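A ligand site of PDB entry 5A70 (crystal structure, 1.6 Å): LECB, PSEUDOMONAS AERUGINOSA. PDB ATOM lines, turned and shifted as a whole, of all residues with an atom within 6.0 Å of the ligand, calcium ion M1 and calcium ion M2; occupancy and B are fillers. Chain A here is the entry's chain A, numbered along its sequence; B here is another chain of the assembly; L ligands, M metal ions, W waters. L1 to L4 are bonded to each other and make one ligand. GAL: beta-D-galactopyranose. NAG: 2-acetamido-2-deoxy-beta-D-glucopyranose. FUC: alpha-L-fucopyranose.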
ATOM      1  N   ASN A  21      17.426 -26.463 -26.813  1.00  0.00           N
ATOM      2  CA  ASN A  21      17.724 -25.090 -26.304  1.00  0.00           C
ATOM      3  C   ASN A  21      16.864 -24.762 -25.110  1.00  0.00           C
ATOM      4  O   ASN A  21      15.923 -23.987 -25.184  1.00  0.00           O
ATOM      5  CB  ASN A  21      17.487 -24.009 -27.366  1.00  0.00           C
ATOM      6  CG  ASN A  21      18.479 -24.029 -28.512  1.00  0.00           C
ATOM      7  OD1 ASN A  21      19.600 -23.600 -28.403  1.00  0.00           O
ATOM      8  ND2 ASN A  21      18.050 -24.608 -29.640  1.00  0.00           N
ATOM      9  N   SER A  22      17.143 -25.419 -23.992  1.00  0.00           N
ATOM     10  CA  SER A  22      16.315 -25.320 -22.819  1.00  0.00           C
ATOM     11  C   SER A  22      17.054 -25.897 -21.615  1.00  0.00           C
ATOM     12  O   SER A  22      17.836 -26.825 -21.784  1.00  0.00           O
ATOM     13  CB  SER A  22      15.032 -26.052 -23.010  1.00  0.00           C
ATOM     14  OG  SER A  22      14.236 -26.075 -21.850  1.00  0.00           O
ATOM     15  N   ALA A  23      16.697 -25.427 -20.443  1.00  0.00           N
ATOM     16  CA  ALA A  23      17.206 -26.082 -19.207  1.00  0.00           C
ATOM     17  C   ALA A  23      16.657 -27.519 -19.055  1.00  0.00           C
ATOM     18  O   ALA A  23      17.280 -28.357 -18.386  1.00  0.00           O
ATOM     19  CB  ALA A  23      16.796 -25.242 -17.996  1.00  0.00           C
ATOM     20  N   GLY A  24      15.487 -27.775 -19.627  1.00  0.00           N
ATOM     21  CA  GLY A  24      14.792 -29.051 -19.480  1.00  0.00           C
ATOM     22  C   GLY A  24      15.238 -30.063 -20.485  1.00  0.00           C
ATOM     23  O   GLY A  24      15.519 -29.756 -21.654  1.00  0.00           O
ATOM     24  N   THR A  25      15.341 -31.318 -20.050  1.00  0.00           N
ATOM     25  CA  THR A  25      15.644 -32.414 -20.947  1.00  0.00           C
ATOM     26  C   THR A  25      14.461 -32.619 -21.914  1.00  0.00           C
ATOM     27  O   THR A  25      13.325 -32.755 -21.487  1.00  0.00           O
ATOM     28  CB  THR A  25      15.906 -33.714 -20.142  1.00  0.00           C
ATOM     29  OG1 THR A  25      17.102 -33.458 -19.332  1.00  0.00           O
ATOM     30  CG2 THR A  25      16.185 -34.888 -21.067  1.00  0.00           C
ATOM     31  N   GLN A  26      14.764 -32.626 -23.182  1.00  0.00           N
ATOM     32  CA  GLN A  26      13.739 -32.777 -24.205  1.00  0.00           C
ATOM     33  C   GLN A  26      13.598 -34.242 -24.587  1.00  0.00           C
ATOM     34  O   GLN A  26      14.603 -34.900 -24.846  1.00  0.00           O
ATOM     35  CB  GLN A  26      14.128 -31.952 -25.443  1.00  0.00           C
ATOM     36  CG  GLN A  26      14.413 -30.504 -25.133  1.00  0.00           C
ATOM     37  CD  GLN A  26      13.200 -29.734 -24.728  1.00  0.00           C
ATOM     38  OE1 GLN A  26      12.181 -29.743 -25.414  1.00  0.00           O
ATOM     39  NE2 GLN A  26      13.303 -29.002 -23.614  1.00  0.00           N
ATOM     40  N   THR A  45      21.452 -25.986 -23.729  1.00  0.00           N
ATOM     41  CA  THR A  45      21.043 -24.584 -23.917  1.00  0.00           C
ATOM     42  C   THR A  45      21.874 -23.937 -25.047  1.00  0.00           C
ATOM     43  O   THR A  45      21.919 -22.707 -25.182  1.00  0.00           O
ATOM     44  CB  THR A  45      21.120 -23.757 -22.637  1.00  0.00           C
ATOM     45  OG1 THR A  45      22.425 -23.924 -22.031  1.00  0.00           O
ATOM     46  CG2 THR A  45      20.036 -24.121 -21.684  1.00  0.00           C
ATOM     47  N   VAL A  69       8.619 -32.644 -22.064  1.00  0.00           N
ATOM     48  CA  VAL A  69       9.697 -32.356 -21.122  1.00  0.00           C
ATOM     49  C   VAL A  69       9.178 -32.800 -19.781  1.00  0.00           C
ATOM     50  O   VAL A  69       8.190 -32.281 -19.292  1.00  0.00           O
ATOM     51  CB  VAL A  69      10.036 -30.868 -21.044  1.00  0.00           C
ATOM     52  CG1 VAL A  69      11.127 -30.657 -19.971  1.00  0.00           C
ATOM     53  CG2 VAL A  69      10.470 -30.377 -22.376  1.00  0.00           C
ATOM     54  N   SER A  94       9.125 -25.920 -30.658  1.00  0.00           N
ATOM     55  CA  SER A  94       8.358 -26.321 -29.485  1.00  0.00           C
ATOM     56  C   SER A  94       8.674 -25.447 -28.289  1.00  0.00           C
ATOM     57  O   SER A  94       9.799 -24.979 -28.163  1.00  0.00           O
ATOM     58  CB  SER A  94       8.575 -27.802 -29.173  1.00  0.00           C
ATOM     59  OG  SER A  94       9.926 -28.077 -28.777  1.00  0.00           O
ATOM     60  N   GLU A  95       7.697 -25.311 -27.422  1.00  0.00           N
ATOM     61  CA  GLU A  95       7.826 -24.447 -26.269  1.00  0.00           C
ATOM     62  C   GLU A  95       7.401 -25.190 -25.035  1.00  0.00           C
ATOM     63  O   GLU A  95       6.276 -25.670 -24.960  1.00  0.00           O
ATOM     64  CB  GLU A  95       6.949 -23.222 -26.464  1.00  0.00           C
ATOM     65  CG  GLU A  95       6.976 -22.257 -25.299  1.00  0.00           C
ATOM     66  CD  GLU A  95       8.370 -21.823 -24.877  1.00  0.00           C
ATOM     67  OE1 GLU A  95       9.175 -21.361 -25.722  1.00  0.00           O
ATOM     68  OE2 GLU A  95       8.740 -22.025 -23.678  1.00  0.00           O
ATOM     69  N   ASP A  96       8.343 -25.289 -24.093  1.00  0.00           N
ATOM     70  CA  ASP A  96       8.148 -26.006 -22.822  1.00  0.00           C
ATOM     71  C   ASP A  96       7.818 -25.146 -21.628  1.00  0.00           C
ATOM     72  O   ASP A  96       7.633 -25.689 -20.503  1.00  0.00           O
ATOM     73  CB  ASP A  96       9.376 -26.894 -22.501  1.00  0.00           C
ATOM     74  CG  ASP A  96      10.650 -26.137 -22.290  1.00  0.00           C
ATOM     75  OD1 ASP A  96      10.585 -25.004 -21.783  1.00  0.00           O
ATOM     76  OD2 ASP A  96      11.728 -26.724 -22.478  1.00  0.00           O
ATOM     77  N   SER A  97       7.669 -23.858 -21.829  1.00  0.00           N
ATOM     78  CA  SER A  97       7.516 -22.903 -20.739  1.00  0.00           C
ATOM     79  C   SER A  97       6.725 -21.700 -21.218  1.00  0.00           C
ATOM     80  O   SER A  97       5.806 -21.875 -22.047  1.00  0.00           O
ATOM     81  CB  SER A  97       8.907 -22.533 -20.254  1.00  0.00           C
ATOM     82  OG  SER A  97       8.837 -21.731 -19.054  1.00  0.00           O
ATOM     83  N   THR A  98       7.045 -20.510 -20.731  1.00  0.00           N
ATOM     84  CA  THR A  98       6.288 -19.326 -20.961  1.00  0.00           C
ATOM     85  C   THR A  98       6.984 -18.201 -21.725  1.00  0.00           C
ATOM     86  O   THR A  98       6.352 -17.205 -22.035  1.00  0.00           O
ATOM     87  CB  THR A  98       5.822 -18.678 -19.620  1.00  0.00           C
ATOM     88  OG1 THR A  98       6.961 -18.491 -18.796  1.00  0.00           O
ATOM     89  CG2 THR A  98       4.862 -19.590 -18.901  1.00  0.00           C
ATOM     90  N   ASP A  99       8.274 -18.359 -22.048  1.00  0.00           N
ATOM     91  CA  ASP A  99       8.985 -17.297 -22.732  1.00  0.00           C
ATOM     92  C   ASP A  99       8.712 -17.237 -24.235  1.00  0.00           C
ATOM     93  O   ASP A  99       9.108 -16.286 -24.876  1.00  0.00           O
ATOM     94  CB  ASP A  99      10.501 -17.323 -22.446  1.00  0.00           C
ATOM     95  CG  ASP A  99      11.215 -18.558 -22.975  1.00  0.00           C
ATOM     96  OD1 ASP A  99      10.546 -19.575 -23.206  1.00  0.00           O
ATOM     97  OD2 ASP A  99      12.465 -18.497 -23.102  1.00  0.00           O
ATOM     98  N   ASN A 100       8.151 -18.306 -24.797  1.00  0.00           N
ATOM     99  CA  ASN A 100       7.735 -18.371 -26.196  1.00  0.00           C
ATOM    100  C   ASN A 100       8.854 -18.161 -27.180  1.00  0.00           C
ATOM    101  O   ASN A 100       8.690 -17.488 -28.201  1.00  0.00           O
ATOM    102  CB  ASN A 100       6.568 -17.433 -26.407  1.00  0.00           C
ATOM    103  CG  ASN A 100       5.353 -17.879 -25.619  1.00  0.00           C
ATOM    104  OD1 ASN A 100       5.240 -19.038 -25.216  1.00  0.00           O
ATOM    105  ND2 ASN A 100       4.436 -16.999 -25.401  1.00  0.00           N
ATOM    106  N   ASP A 101      10.029 -18.701 -26.866  1.00  0.00           N
ATOM    107  CA  ASP A 101      11.110 -18.684 -27.852  1.00  0.00           C
ATOM    108  C   ASP A 101      10.914 -19.825 -28.886  1.00  0.00           C
ATOM    109  O   ASP A 101      11.497 -19.802 -29.952  1.00  0.00           O
ATOM    110  CB  ASP A 101      12.492 -18.598 -27.237  1.00  0.00           C
ATOM    111  CG  ASP A 101      12.872 -19.752 -26.325  1.00  0.00           C
ATOM    112  OD1 ASP A 101      12.047 -20.658 -26.002  1.00  0.00           O
ATOM    113  OD2 ASP A 101      14.090 -19.761 -25.947  1.00  0.00           O
ATOM    114  N   TYR A 102      10.105 -20.830 -28.523  1.00  0.00           N
ATOM    115  CA  TYR A 102       9.757 -21.953 -29.452  1.00  0.00           C
ATOM    116  C   TYR A 102      10.980 -22.690 -29.984  1.00  0.00           C
ATOM    117  O   TYR A 102      10.900 -23.384 -31.005  1.00  0.00           O
ATOM    118  CB  TYR A 102       8.777 -21.517 -30.586  1.00  0.00           C
ATOM    119  CG  TYR A 102       7.387 -21.484 -30.054  1.00  0.00           C
ATOM    120  CD1 TYR A 102       6.607 -22.604 -30.076  1.00  0.00           C
ATOM    121  CD2 TYR A 102       6.878 -20.357 -29.467  1.00  0.00           C
ATOM    122  CE1 TYR A 102       5.338 -22.615 -29.520  1.00  0.00           C
ATOM    123  CE2 TYR A 102       5.606 -20.377 -28.896  1.00  0.00           C
ATOM    124  CZ  TYR A 102       4.893 -21.500 -28.918  1.00  0.00           C
ATOM    125  OH  TYR A 102       3.647 -21.467 -28.306  1.00  0.00           O
ATOM    126  N   ASN A 103      12.119 -22.618 -29.266  1.00  0.00           N
ATOM    127  CA  ASN A 103      13.321 -23.325 -29.670  1.00  0.00           C
ATOM    128  C   ASN A 103      13.735 -24.472 -28.716  1.00  0.00           C
ATOM    129  O   ASN A 103      14.817 -24.990 -28.878  1.00  0.00           O
ATOM    130  CB  ASN A 103      14.489 -22.369 -29.827  1.00  0.00           C
ATOM    131  CG  ASN A 103      14.993 -21.873 -28.476  1.00  0.00           C
ATOM    132  OD1 ASN A 103      14.419 -22.216 -27.452  1.00  0.00           O
ATOM    133  ND2 ASN A 103      16.031 -21.094 -28.476  1.00  0.00           N
ATOM    134  N   ASP A 104      12.862 -24.822 -27.796  1.00  0.00           N
ATOM    135  CA  ASP A 104      13.290 -25.656 -26.673  1.00  0.00           C
ATOM    136  C   ASP A 104      13.696 -27.038 -27.186  1.00  0.00           C
ATOM    137  O   ASP A 104      14.719 -27.581 -26.792  1.00  0.00           O
ATOM    138  CB  ASP A 104      12.188 -25.682 -25.621  1.00  0.00           C
ATOM    139  CG  ASP A 104      11.885 -24.322 -25.055  1.00  0.00           C
ATOM    140  OD1 ASP A 104      12.863 -23.504 -24.920  1.00  0.00           O
ATOM    141  OD2 ASP A 104      10.755 -24.001 -24.758  1.00  0.00           O
ATOM    142  N   LEU B 113      18.891 -19.074 -30.144  1.00  0.00           N
ATOM    143  CA  LEU B 113      19.359 -20.176 -29.333  1.00  0.00           C
ATOM    144  C   LEU B 113      19.077 -19.911 -27.881  1.00  0.00           C
ATOM    145  O   LEU B 113      18.731 -18.828 -27.486  1.00  0.00           O
ATOM    146  CB  LEU B 113      20.856 -20.422 -29.559  1.00  0.00           C
ATOM    147  CG  LEU B 113      21.348 -20.614 -30.956  1.00  0.00           C
ATOM    148  CD1 LEU B 113      22.810 -21.069 -30.992  1.00  0.00           C
ATOM    149  CD2 LEU B 113      20.470 -21.658 -31.665  1.00  0.00           C
ATOM    150  N   GLY B 114      19.324 -20.922 -27.078  1.00  0.00           N
ATOM    151  CA  GLY B 114      19.303 -20.785 -25.633  1.00  0.00           C
ATOM    152  C   GLY B 114      17.969 -21.036 -24.962  1.00  0.00           C
ATOM    153  O   GLY B 114      16.922 -21.077 -25.596  1.00  0.00           O
ATOM    154  OXT GLY B 114      18.024 -21.216 -23.724  1.00  0.00           O
HETATM  155  C1  GAL L   1       9.876 -27.437 -13.592  1.00  0.00           C
HETATM  156  C2  GAL L   1       9.772 -26.350 -14.661  1.00  0.00           C
HETATM  157  C3  GAL L   1      11.051 -25.554 -14.628  1.00  0.00           C
HETATM  158  C4  GAL L   1      11.356 -25.000 -13.229  1.00  0.00           C
HETATM  159  C5  GAL L   1      11.363 -26.171 -12.254  1.00  0.00           C
HETATM  160  C6  GAL L   1      11.670 -25.780 -10.801  1.00  0.00           C
HETATM  161  O1  GAL L   1       8.590 -28.034 -13.652  1.00  0.00           O
HETATM  162  O2  GAL L   1       9.538 -26.969 -15.961  1.00  0.00           O
HETATM  163  O3  GAL L   1      10.886 -24.488 -15.603  1.00  0.00           O
HETATM  164  O4  GAL L   1      10.331 -24.050 -12.918  1.00  0.00           O
HETATM  165  O5  GAL L   1      10.068 -26.766 -12.341  1.00  0.00           O
HETATM  166  O6  GAL L   1      11.953 -27.025 -10.096  1.00  0.00           O
HETATM  167  C1  NAG L   2      12.094 -23.937 -16.029  1.00  0.00           C
HETATM  168  C2  NAG L   2      11.909 -23.539 -17.513  1.00  0.00           C
HETATM  169  C3  NAG L   2      13.201 -22.868 -17.980  1.00  0.00           C
HETATM  170  C4  NAG L   2      13.560 -21.709 -17.030  1.00  0.00           C
HETATM  171  C5  NAG L   2      13.676 -22.233 -15.600  1.00  0.00           C
HETATM  172  C6  NAG L   2      13.981 -21.210 -14.501  1.00  0.00           C
HETATM  173  C7  NAG L   2      12.243 -25.778 -18.383  1.00  0.00           C
HETATM  174  C8  NAG L   2      11.565 -26.915 -19.053  1.00  0.00           C
HETATM  175  N2  NAG L   2      11.481 -24.720 -18.211  1.00  0.00           N
HETATM  176  O3  NAG L   2      12.992 -22.309 -19.295  1.00  0.00           O
HETATM  177  O4  NAG L   2      14.842 -21.201 -17.424  1.00  0.00           O
HETATM  178  O5  NAG L   2      12.408 -22.791 -15.259  1.00  0.00           O
HETATM  179  O6  NAG L   2      12.950 -20.233 -14.537  1.00  0.00           O
HETATM  180  O7  NAG L   2      13.426 -25.853 -18.088  1.00  0.00           O
HETATM  181  C1  FUC L   3      13.585 -23.081 -20.262  1.00  0.00           C
HETATM  182  C2  FUC L   3      13.119 -22.667 -21.659  1.00  0.00           C
HETATM  183  C3  FUC L   3      13.639 -21.259 -21.946  1.00  0.00           C
HETATM  184  C4  FUC L   3      15.120 -21.237 -21.832  1.00  0.00           C
HETATM  185  C5  FUC L   3      15.570 -21.776 -20.462  1.00  0.00           C
HETATM  186  C6  FUC L   3      17.073 -21.857 -20.304  1.00  0.00           C
HETATM  187  O2  FUC L   3      11.743 -22.695 -21.898  1.00  0.00           O
HETATM  188  O3  FUC L   3      13.239 -20.898 -23.332  1.00  0.00           O
HETATM  189  O4  FUC L   3      15.715 -21.968 -22.909  1.00  0.00           O
HETATM  190  O5  FUC L   3      14.973 -23.057 -20.259  1.00  0.00           O
HETATM  191  C1  GAL L   4      14.875 -19.795 -17.393  1.00  0.00           C
HETATM  192  C2  GAL L   4      16.328 -19.355 -17.483  1.00  0.00           C
HETATM  193  C3  GAL L   4      16.463 -17.851 -17.649  1.00  0.00           C
HETATM  194  C4  GAL L   4      15.652 -17.394 -18.831  1.00  0.00           C
HETATM  195  C5  GAL L   4      14.224 -17.842 -18.614  1.00  0.00           C
HETATM  196  C6  GAL L   4      13.293 -17.514 -19.751  1.00  0.00           C
HETATM  197  O2  GAL L   4      17.031 -19.702 -16.272  1.00  0.00           O
HETATM  198  O3  GAL L   4      17.850 -17.602 -17.912  1.00  0.00           O
HETATM  199  O4  GAL L   4      16.290 -17.966 -19.992  1.00  0.00           O
HETATM  200  O5  GAL L   4      14.124 -19.263 -18.476  1.00  0.00           O
HETATM  201  O6  GAL L   4      11.949 -17.725 -19.320  1.00  0.00           O
HETATM  202 CA    CA M   1      11.070 -21.735 -24.132  1.00  0.00          CA
HETATM  203 CA    CA M   2      14.650 -21.954 -25.124  1.00  0.00          CA
HETATM  204  O   HOH W   1      14.319 -27.784 -16.272  1.00  0.00           O
HETATM  205  O   HOH W   2       9.180 -21.608 -14.847  1.00  0.00           O
HETATM  206  O   HOH W   3      14.237 -28.865 -10.822  1.00  0.00           O
HETATM  207  O   HOH W   4      10.670 -29.630 -16.450  1.00  0.00           O
HETATM  208  O   HOH W   5      18.039 -22.302 -16.117  1.00  0.00           O
HETATM  209  O   HOH W   6      20.456 -19.092 -17.723  1.00  0.00           O
HETATM  210  O   HOH W   7      11.103 -20.185 -19.381  1.00  0.00           O
HETATM  211  O   HOH W   8       8.374 -26.187  -9.841  1.00  0.00           O
HETATM  212  O   HOH W   9       9.707 -28.274  -9.133  1.00  0.00           O
HETATM  213  O   HOH W  10      18.194 -14.932 -17.982  1.00  0.00           O
HETATM  214  O   HOH W  11       8.683 -25.147 -17.956  1.00  0.00           O
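O2 of FUC L3 sits close to OD1 of Asp 96 (2.6 Å). The side-chain hydroxyl (OG) of Ser 22 lies close to an oxygen (O5) of FUC L3 (3.5 Å). An oxygen (O5) of FUC L3 sits at hydrogen-bond distance from the backbone NH (N) of Ala 23, at 2.9 Å. The backbone NH (N) of Gly 24 sits at hydrogen-bond distance from an oxygen (O7) of NAG L2.
The nearest printed residue that does not touch calcium ion M2 is Ser 22 (4.4 Å).
CG2 of Thr 45 touches C6 of FUC L3, 3.98 Å away. CG1 of Val 69 touches C8 of NAG L2, 3.9 Å away. CB of Ser 97 touches O2 of FUC L3, 3.3 Å away. 13 residues have an atom within 4 Å of the ligand: Asn 21, Ser 22, Ala 23, Gly 24, Thr 45, Val 69, Glu 95, Asp 96, Ser 97, Asp 99, Asp 101, Asp 104 and Gly 114 of chain B. Along chain A the residues within 4 Å of the ligand span positions 21 to 104.
Calcium ion M1 is bound by the side-chain carboxylate (OD1) of Asp 101 (2.4 Å), the side-chain carboxylate (OD2) of Asp 104 (2.4 Å), the side-chain carboxylate (OE2) of Glu 95 (2.4 Å), the side-chain carboxylate (OD1) of Asp 99 (2.4 Å), an oxygen (O3) of FUC L3 (2.5 Å), the side-chain carboxylate (OE1) of Glu 95 (2.5 Å), an oxygen (O2) of FUC L3 (2.5 Å) and the side-chain carboxylate (OD1) of Asp 104 (2.6 Å).
OD1 of Asn 103 binds calcium ion M2 (2.4 Å). Calcium ion M2 is bound by OD1 of Asp 104 (2.4 Å). Calcium ion M2 is bound by the backbone carbonyl oxygen (O) of Asn 21, 2.4 Å away. The side-chain carboxylate (OD2) of Asp 101 is bound to calcium ion M2 (2.4 Å). Calcium ion M2 is bound by O4 of FUC L3 (2.5 Å). The chain-end carboxylate (O) of Gly 114 of chain B is bound to calcium ion M2 (2.5 Å). O3 of FUC L3 is bound to calcium ion M2, at 2.5 Å. Calcium ion M2 has seven donor atoms within binding distance. Slightly farther from calcium ion M2 lies the side-chain carboxylate (OD1) of Asp 101 (3.0 Å).
Four residues have an atom within 4 Å of calcium ion M1: Glu 95, Asp 99, Asp 101 and Asp 104. The nearest printed residue that does not touch calcium ion M1 is Asp 96 (4.1 Å).
Water W7 lies within hydrogen-bond range of O6 of GAL L4 (2.6 Å) and OG of Ser 97 (2.8 Å). Water W11 bridges the backbone carbonyl oxygen of Asp 96 (2.8 Å) and an oxygen (O2) of GAL L1 (2.8 Å).
N of Asn 103 lies within hydrogen-bond range of O of Ser 94, at 3.5 Å. The side-chain carboxylate of Glu 95 sits close to the backbone NH of Ser 97 (2.8 Å). The backbone NH (N) of Asp 104 sits at hydrogen-bond distance from the backbone carbonyl oxygen (O) of Ser 94, 3.1 Å away. N of Asn 100 lies close to OE1 of Glu 95. The side-chain amide nitrogen (NE2) of Gln 26 is in hydrogen-bond range of the backbone carbonyl oxygen (O) of Gly 24, 3.1 Å away. The backbone NH of Gly 24 sits at hydrogen-bond distance from the side-chain hydroxyl of Ser 22. OE1 of Glu 95 sits close to N of Tyr 102, 3.0 Å away. The side-chain carboxylate (OD2) of Asp 96 lies within hydrogen-bond range of the side-chain amide nitrogen (NE2) of Gln 26 (3.0 Å).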
